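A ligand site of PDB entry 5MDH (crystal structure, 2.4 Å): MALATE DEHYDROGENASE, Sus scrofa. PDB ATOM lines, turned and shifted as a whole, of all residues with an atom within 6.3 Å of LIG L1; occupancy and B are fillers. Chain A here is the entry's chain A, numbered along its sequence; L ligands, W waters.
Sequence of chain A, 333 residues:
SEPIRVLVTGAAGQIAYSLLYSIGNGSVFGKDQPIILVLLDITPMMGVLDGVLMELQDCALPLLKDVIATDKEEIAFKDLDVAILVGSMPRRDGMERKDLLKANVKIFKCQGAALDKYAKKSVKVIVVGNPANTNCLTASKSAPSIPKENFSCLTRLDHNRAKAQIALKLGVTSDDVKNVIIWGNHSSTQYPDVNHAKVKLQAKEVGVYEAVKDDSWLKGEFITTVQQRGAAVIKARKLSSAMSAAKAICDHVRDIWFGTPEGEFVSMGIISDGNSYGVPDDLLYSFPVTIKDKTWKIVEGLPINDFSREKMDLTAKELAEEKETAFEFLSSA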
ATOM      1  N   ARG A  91     -13.520  16.850 -28.467  1.00  0.00           N
ATOM      2  CA  ARG A  91     -13.627  16.378 -29.859  1.00  0.00           C
ATOM      3  C   ARG A  91     -13.140  14.932 -29.869  1.00  0.00           C
ATOM      4  O   ARG A  91     -12.568  14.524 -28.866  1.00  0.00           O
ATOM      5  CB  ARG A  91     -12.819  17.252 -30.807  1.00  0.00           C
ATOM      6  CG  ARG A  91     -11.367  17.418 -30.402  1.00  0.00           C
ATOM      7  CD  ARG A  91     -10.492  17.661 -31.623  1.00  0.00           C
ATOM      8  NE  ARG A  91      -9.156  18.032 -31.157  1.00  0.00           N
ATOM      9  CZ  ARG A  91      -8.087  18.267 -31.898  1.00  0.00           C
ATOM     10  NH1 ARG A  91      -8.199  18.186 -33.198  1.00  0.00           N
ATOM     11  NH2 ARG A  91      -6.920  18.609 -31.335  1.00  0.00           N
ATOM     12  N   ARG A  97     -10.619  21.240 -33.731  1.00  0.00           N
ATOM     13  CA  ARG A  97     -11.263  21.934 -32.612  1.00  0.00           C
ATOM     14  C   ARG A  97     -12.491  22.745 -33.045  1.00  0.00           C
ATOM     15  O   ARG A  97     -13.454  22.854 -32.279  1.00  0.00           O
ATOM     16  CB  ARG A  97     -10.243  22.759 -31.825  1.00  0.00           C
ATOM     17  CG  ARG A  97      -9.186  21.900 -31.129  1.00  0.00           C
ATOM     18  CD  ARG A  97      -8.290  22.646 -30.165  1.00  0.00           C
ATOM     19  NE  ARG A  97      -7.017  22.044 -29.864  1.00  0.00           N
ATOM     20  CZ  ARG A  97      -5.954  21.642 -30.524  1.00  0.00           C
ATOM     21  NH1 ARG A  97      -5.870  21.760 -31.834  1.00  0.00           N
ATOM     22  NH2 ARG A  97      -4.897  21.086 -29.931  1.00  0.00           N
ATOM     23  N   LEU A 100     -17.451  21.753 -32.480  1.00  0.00           N
ATOM     24  CA  LEU A 100     -17.510  21.787 -31.046  1.00  0.00           C
ATOM     25  C   LEU A 100     -17.894  23.258 -30.785  1.00  0.00           C
ATOM     26  O   LEU A 100     -18.578  23.536 -29.822  1.00  0.00           O
ATOM     27  CB  LEU A 100     -16.275  21.419 -30.269  1.00  0.00           C
ATOM     28  CG  LEU A 100     -15.742  19.993 -30.173  1.00  0.00           C
ATOM     29  CD1 LEU A 100     -14.536  19.903 -29.233  1.00  0.00           C
ATOM     30  CD2 LEU A 100     -16.834  19.033 -29.797  1.00  0.00           C
ATOM     31  N   VAL A 128     -10.434  26.707 -20.905  1.00  0.00           N
ATOM     32  CA  VAL A 128      -9.811  25.540 -21.501  1.00  0.00           C
ATOM     33  C   VAL A 128     -10.672  24.846 -22.548  1.00  0.00           C
ATOM     34  O   VAL A 128     -10.201  24.514 -23.635  1.00  0.00           O
ATOM     35  CB  VAL A 128      -9.425  24.479 -20.430  1.00  0.00           C
ATOM     36  CG1 VAL A 128      -8.640  23.362 -21.111  1.00  0.00           C
ATOM     37  CG2 VAL A 128      -8.630  25.122 -19.301  1.00  0.00           C
ATOM     38  N   ASN A 130     -12.794  23.605 -25.705  1.00  0.00           N
ATOM     39  CA  ASN A 130     -12.635  23.957 -27.098  1.00  0.00           C
ATOM     40  C   ASN A 130     -13.760  24.681 -27.773  1.00  0.00           C
ATOM     41  O   ASN A 130     -14.692  23.921 -27.545  1.00  0.00           O
ATOM     42  CB  ASN A 130     -12.122  22.765 -27.924  1.00  0.00           C
ATOM     43  CG  ASN A 130     -10.667  22.546 -27.485  1.00  0.00           C
ATOM     44  OD1 ASN A 130     -10.263  21.409 -27.224  1.00  0.00           O
ATOM     45  ND2 ASN A 130      -9.912  23.652 -27.415  1.00  0.00           N
ATOM     46  N   LEU A 154      -6.234  28.985 -22.507  1.00  0.00           N
ATOM     47  CA  LEU A 154      -5.044  28.153 -22.444  1.00  0.00           C
ATOM     48  C   LEU A 154      -4.312  27.796 -23.702  1.00  0.00           C
ATOM     49  O   LEU A 154      -4.776  26.947 -24.477  1.00  0.00           O
ATOM     50  CB  LEU A 154      -5.439  26.822 -21.764  1.00  0.00           C
ATOM     51  CG  LEU A 154      -4.324  25.895 -21.307  1.00  0.00           C
ATOM     52  CD1 LEU A 154      -3.760  26.308 -19.937  1.00  0.00           C
ATOM     53  CD2 LEU A 154      -4.856  24.458 -21.225  1.00  0.00           C
ATOM     54  N   LEU A 157      -0.474  24.638 -22.732  1.00  0.00           N
ATOM     55  CA  LEU A 157      -0.198  23.253 -23.115  1.00  0.00           C
ATOM     56  C   LEU A 157       0.608  23.222 -24.397  1.00  0.00           C
ATOM     57  O   LEU A 157       1.559  22.424 -24.541  1.00  0.00           O
ATOM     58  CB  LEU A 157      -1.482  22.436 -23.180  1.00  0.00           C
ATOM     59  CG  LEU A 157      -1.335  20.968 -23.565  1.00  0.00           C
ATOM     60  CD1 LEU A 157      -0.143  20.313 -22.925  1.00  0.00           C
ATOM     61  CD2 LEU A 157      -2.644  20.227 -23.184  1.00  0.00           C
ATOM     62  N   ASP A 158       0.272  24.058 -25.373  1.00  0.00           N
ATOM     63  CA  ASP A 158       1.013  24.138 -26.629  1.00  0.00           C
ATOM     64  C   ASP A 158       2.418  24.689 -26.319  1.00  0.00           C
ATOM     65  O   ASP A 158       3.381  24.276 -26.910  1.00  0.00           O
ATOM     66  CB  ASP A 158       0.371  25.048 -27.671  1.00  0.00           C
ATOM     67  CG  ASP A 158      -1.098  24.841 -27.942  1.00  0.00           C
ATOM     68  OD1 ASP A 158      -1.493  23.679 -28.246  1.00  0.00           O
ATOM     69  OD2 ASP A 158      -1.883  25.820 -27.871  1.00  0.00           O
ATOM     70  N   ARG A 161       4.347  21.934 -24.810  1.00  0.00           N
ATOM     71  CA  ARG A 161       4.637  20.977 -25.875  1.00  0.00           C
ATOM     72  C   ARG A 161       5.800  21.433 -26.754  1.00  0.00           C
ATOM     73  O   ARG A 161       6.556  20.550 -27.209  1.00  0.00           O
ATOM     74  CB  ARG A 161       3.431  20.719 -26.806  1.00  0.00           C
ATOM     75  CG  ARG A 161       2.358  19.886 -26.104  1.00  0.00           C
ATOM     76  CD  ARG A 161       1.018  19.999 -26.803  1.00  0.00           C
ATOM     77  NE  ARG A 161       0.088  18.952 -26.438  1.00  0.00           N
ATOM     78  CZ  ARG A 161      -1.224  18.975 -26.710  1.00  0.00           C
ATOM     79  NH1 ARG A 161      -1.776  20.020 -27.366  1.00  0.00           N
ATOM     80  NH2 ARG A 161      -1.955  17.955 -26.298  1.00  0.00           N
ATOM     81  N   HIS A 186      -5.505  28.469 -30.316  1.00  0.00           N
ATOM     82  CA  HIS A 186      -5.244  27.150 -29.745  1.00  0.00           C
ATOM     83  C   HIS A 186      -5.820  26.141 -30.733  1.00  0.00           C
ATOM     84  O   HIS A 186      -6.938  25.643 -30.560  1.00  0.00           O
ATOM     85  CB  HIS A 186      -5.887  27.016 -28.343  1.00  0.00           C
ATOM     86  CG  HIS A 186      -5.653  25.640 -27.823  1.00  0.00           C
ATOM     87  ND1 HIS A 186      -4.356  25.129 -27.824  1.00  0.00           N
ATOM     88  CD2 HIS A 186      -6.477  24.656 -27.397  1.00  0.00           C
ATOM     89  CE1 HIS A 186      -4.382  23.894 -27.369  1.00  0.00           C
ATOM     90  NE2 HIS A 186      -5.653  23.598 -27.142  1.00  0.00           N
ATOM     91  N   GLY A 230      -2.297  17.724 -30.186  1.00  0.00           N
ATOM     92  CA  GLY A 230      -3.557  17.365 -29.530  1.00  0.00           C
ATOM     93  C   GLY A 230      -4.266  16.236 -30.244  1.00  0.00           C
ATOM     94  O   GLY A 230      -4.765  15.303 -29.583  1.00  0.00           O
ATOM     95  N   ALA A 231      -4.319  16.297 -31.574  1.00  0.00           N
ATOM     96  CA  ALA A 231      -4.885  15.279 -32.425  1.00  0.00           C
ATOM     97  C   ALA A 231      -4.128  13.965 -32.340  1.00  0.00           C
ATOM     98  O   ALA A 231      -4.755  12.874 -32.364  1.00  0.00           O
ATOM     99  CB  ALA A 231      -4.923  15.807 -33.856  1.00  0.00           C
ATOM    100  N   VAL A 233      -2.521  12.829 -29.652  1.00  0.00           N
ATOM    101  CA  VAL A 233      -2.751  12.233 -28.331  1.00  0.00           C
ATOM    102  C   VAL A 233      -4.078  11.484 -28.342  1.00  0.00           C
ATOM    103  O   VAL A 233      -4.212  10.355 -27.862  1.00  0.00           O
ATOM    104  CB  VAL A 233      -2.665  13.313 -27.237  1.00  0.00           C
ATOM    105  CG1 VAL A 233      -3.173  12.779 -25.899  1.00  0.00           C
ATOM    106  CG2 VAL A 233      -1.236  13.814 -27.112  1.00  0.00           C
ATOM    107  N   ILE A 234      -5.112  12.081 -28.918  1.00  0.00           N
ATOM    108  CA  ILE A 234      -6.474  11.581 -29.033  1.00  0.00           C
ATOM    109  C   ILE A 234      -6.461  10.329 -29.915  1.00  0.00           C
ATOM    110  O   ILE A 234      -7.166   9.367 -29.680  1.00  0.00           O
ATOM    111  CB  ILE A 234      -7.424  12.597 -29.681  1.00  0.00           C
ATOM    112  CG1 ILE A 234      -7.780  13.785 -28.783  1.00  0.00           C
ATOM    113  CG2 ILE A 234      -8.722  11.920 -30.149  1.00  0.00           C
ATOM    114  CD1 ILE A 234      -8.173  14.987 -29.666  1.00  0.00           C
ATOM    115  N   SER A 240      -8.975  12.685 -25.035  1.00  0.00           N
ATOM    116  CA  SER A 240      -8.304  13.964 -25.119  1.00  0.00           C
ATOM    117  C   SER A 240      -7.184  13.957 -24.079  1.00  0.00           C
ATOM    118  O   SER A 240      -7.039  13.024 -23.283  1.00  0.00           O
ATOM    119  CB  SER A 240      -9.348  15.080 -24.998  1.00  0.00           C
ATOM    120  OG  SER A 240      -9.187  15.924 -23.871  1.00  0.00           O
ATOM    121  N   SER A 241      -6.256  14.890 -24.193  1.00  0.00           N
ATOM    122  CA  SER A 241      -5.131  14.914 -23.243  1.00  0.00           C
ATOM    123  C   SER A 241      -5.766  15.341 -21.933  1.00  0.00           C
ATOM    124  O   SER A 241      -6.807  16.031 -22.057  1.00  0.00           O
ATOM    125  CB  SER A 241      -4.123  15.930 -23.778  1.00  0.00           C
ATOM    126  OG  SER A 241      -4.457  17.216 -23.285  1.00  0.00           O
ATOM    127  N   ALA A 242      -5.254  15.031 -20.773  1.00  0.00           N
ATOM    128  CA  ALA A 242      -5.858  15.430 -19.508  1.00  0.00           C
ATOM    129  C   ALA A 242      -4.757  15.668 -18.486  1.00  0.00           C
ATOM    130  O   ALA A 242      -4.647  16.678 -17.796  1.00  0.00           O
ATOM    131  CB  ALA A 242      -6.879  14.389 -19.048  1.00  0.00           C
ATOM    132  N   SER A 244      -1.550  16.155 -19.147  1.00  0.00           N
ATOM    133  CA  SER A 244      -0.744  17.246 -19.672  1.00  0.00           C
ATOM    134  C   SER A 244      -1.535  18.551 -19.750  1.00  0.00           C
ATOM    135  O   SER A 244      -0.976  19.644 -19.636  1.00  0.00           O
ATOM    136  CB  SER A 244      -0.161  16.819 -21.020  1.00  0.00           C
ATOM    137  OG  SER A 244      -1.125  16.522 -22.015  1.00  0.00           O
ATOM    138  N   ALA A 245      -2.848  18.436 -19.876  1.00  0.00           N
ATOM    139  CA  ALA A 245      -3.735  19.597 -19.933  1.00  0.00           C
ATOM    140  C   ALA A 245      -3.869  20.246 -18.551  1.00  0.00           C
ATOM    141  O   ALA A 245      -3.693  21.446 -18.389  1.00  0.00           O
ATOM    142  CB  ALA A 245      -5.092  19.203 -20.511  1.00  0.00           C
HETATM  143  C1  LIG L   1      -7.578  18.784 -27.476  1.00  0.00           C
HETATM  144  O1  LIG L   1      -7.399  17.563 -27.528  1.00  0.00           O
HETATM  145  O2  LIG L   1      -8.610  19.426 -28.115  1.00  0.00           O
HETATM  146  C2  LIG L   1      -6.685  19.756 -26.706  1.00  0.00           C
HETATM  147  O3  LIG L   1      -6.939  20.954 -26.719  1.00  0.00           O
HETATM  148  C3  LIG L   1      -5.479  19.242 -25.926  1.00  0.00           C
HETATM  149  O4  LIG L   1      -5.338  18.067 -25.564  1.00  0.00           O
HETATM  150  O5  LIG L   1      -4.558  20.223 -25.683  1.00  0.00           O
HETATM  151  P1  LG2 L   2     -14.396  14.925 -20.383  1.00  0.00           P
HETATM  152  O1  LG2 L   2     -14.112  13.670 -19.634  1.00  0.00           O
HETATM  153  O2  LG2 L   2     -15.528  14.711 -21.317  1.00  0.00           O
HETATM  154  O3  LG2 L   2     -14.715  16.064 -19.314  1.00  0.00           O
HETATM  155  C1  LG2 L   2     -15.737  17.069 -19.578  1.00  0.00           C
HETATM  156  C2  LG2 L   2     -16.675  17.283 -18.425  1.00  0.00           C
HETATM  157  O4  LG2 L   2     -17.495  18.448 -18.757  1.00  0.00           O
HETATM  158  C3  LG2 L   2     -17.644  16.148 -18.072  1.00  0.00           C
HETATM  159  O5  LG2 L   2     -17.711  15.811 -16.698  1.00  0.00           O
HETATM  160  C4  LG2 L   2     -19.010  16.716 -18.487  1.00  0.00           C
HETATM  161  O6  LG2 L   2     -20.111  16.115 -17.873  1.00  0.00           O
HETATM  162  C5  LG2 L   2     -18.766  18.194 -18.151  1.00  0.00           C
HETATM  163  N1  LG2 L   2     -19.721  19.130 -18.760  1.00  0.00           N
HETATM  164  C6  LG2 L   2     -20.259  19.080 -20.011  1.00  0.00           C
HETATM  165  N2  LG2 L   2     -21.078  20.099 -20.253  1.00  0.00           N
HETATM  166  C7  LG2 L   2     -21.049  20.843 -19.091  1.00  0.00           C
HETATM  167  C8  LG2 L   2     -21.700  22.031 -18.734  1.00  0.00           C
HETATM  168  N3  LG2 L   2     -22.534  22.680 -19.544  1.00  0.00           N
HETATM  169  N4  LG2 L   2     -21.447  22.510 -17.478  1.00  0.00           N
HETATM  170  C9  LG2 L   2     -20.574  21.831 -16.663  1.00  0.00           C
HETATM  171  N5  LG2 L   2     -19.935  20.728 -16.917  1.00  0.00           N
HETATM  172  C10 LG2 L   2     -20.215  20.265 -18.154  1.00  0.00           C
HETATM  173  O7  LG2 L   2     -13.168  15.503 -21.218  1.00  0.00           O
HETATM  174  P2  LG2 L   2     -12.285  16.835 -21.107  1.00  0.00           P
HETATM  175  O8  LG2 L   2     -11.039  16.675 -21.883  1.00  0.00           O
HETATM  176  O9  LG2 L   2     -12.040  16.990 -19.647  1.00  0.00           O
HETATM  177  O10 LG2 L   2     -13.271  17.940 -21.717  1.00  0.00           O
HETATM  178  C11 LG2 L   2     -13.016  19.309 -21.359  1.00  0.00           C
HETATM  179  C12 LG2 L   2     -12.680  20.156 -22.559  1.00  0.00           C
HETATM  180  O11 LG2 L   2     -11.307  20.644 -22.477  1.00  0.00           O
HETATM  181  C13 LG2 L   2     -12.845  19.539 -23.950  1.00  0.00           C
HETATM  182  O12 LG2 L   2     -13.419  20.491 -24.844  1.00  0.00           O
HETATM  183  C14 LG2 L   2     -11.379  19.290 -24.348  1.00  0.00           C
HETATM  184  O13 LG2 L   2     -11.246  19.207 -25.773  1.00  0.00           O
HETATM  185  C15 LG2 L   2     -10.784  20.594 -23.789  1.00  0.00           C
HETATM  186  N6  LG2 L   2      -9.332  20.600 -23.700  1.00  0.00           N
HETATM  187  C16 LG2 L   2      -8.684  21.764 -23.956  1.00  0.00           C
HETATM  188  C17 LG2 L   2      -7.318  21.805 -23.875  1.00  0.00           C
HETATM  189  C18 LG2 L   2      -6.388  23.038 -24.120  1.00  0.00           C
HETATM  190  O14 LG2 L   2      -5.178  22.780 -24.236  1.00  0.00           O
HETATM  191  N7  LG2 L   2      -6.954  24.244 -24.205  1.00  0.00           N
HETATM  192  C19 LG2 L   2      -6.539  20.677 -23.563  1.00  0.00           C
HETATM  193  C20 LG2 L   2      -7.295  19.527 -23.342  1.00  0.00           C
HETATM  194  C21 LG2 L   2      -8.663  19.396 -23.383  1.00  0.00           C
HETATM  195  O   HOH W   1      -5.428  15.740 -26.942  1.00  0.00           O
HETATM  196  O   HOH W   2     -10.671  16.836 -26.846  1.00  0.00           O
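The guanidinium group of Arg 161 lies within salt-bridge range of an oxygen (O5) of LIG L1 (3.3 Å). A ring nitrogen (NE2) of His 186 is in hydrogen-bond range of an oxygen (O3) of LIG L1, 3.0 Å away. The side-chain amide oxygen (OD1) of Asn 130 is in hydrogen-bond range of an oxygen (O13) of LG2 L2, at 2.8 Å. O2 of LIG L1 lies within salt-bridge range of NE of Arg 91. The side-chain amide oxygen (OD1) of Asn 130 sits close to an oxygen (O2) of LIG L1, 2.7 Å away. NE2 of His 186 lies within hydrogen-bond range of O14 of LG2 L2 (3.1 Å). O4 of LIG L1 is in hydrogen-bond range of OG of Ser 241, at 2.6 Å. A nitrogen (N7) of LG2 L2 lies close to the backbone carbonyl oxygen (O) of Val 128. An oxygen (O12) of LG2 L2 lies within hydrogen-bond range of the backbone NH of Asn 130, 3.3 Å away. An oxygen (O2) of LIG L1 is in salt-bridge range of the guanidinium group (NE) of Arg 97 (3.5 Å). O of Leu 154 is in hydrogen-bond range of N7 of LG2 L2, at 3.5 Å. The side-chain hydroxyl of Ser 240 lies within hydrogen-bond range of an oxygen (O8) of LG2 L2, at 2.8 Å.
An oxygen (O14) of LG2 L2 sits close to an oxygen (O5) of LIG L1, at 3.0 Å.
NE2 of His 186 is in hydrogen-bond range of NE of Arg 97, at 3.4 Å. The guanidinium group (NH1) of Arg 161 lies within salt-bridge range of the side-chain carboxylate (OD1) of Asp 158, 3.8 Å away. ND1 of His 186 lies within hydrogen-bond range of OD2 of Asp 158 (2.6 Å).
Residues that only touch LIG L1: Leu 157 (3.1 Å) and Ile 234 (3.4 Å). Of the 19 residues printed, 8 come within 4 Å of LIG L1. The nearest printed residue that does not touch LIG L1 is Gly 230 (4.03 Å).
Water W1 lies within hydrogen-bond range of O4 of LIG L1 (2.7 Å), O of Gly 230 (2.8 Å) and N of Ser 241 (3.0 Å). Water W2 lies within hydrogen-bond range of O13 of LG2 L2 (2.7 Å), N of Arg 91 (3.3 Å), O1 of LIG L1 (3.4 Å) and OG of Ser 240 (3.4 Å).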
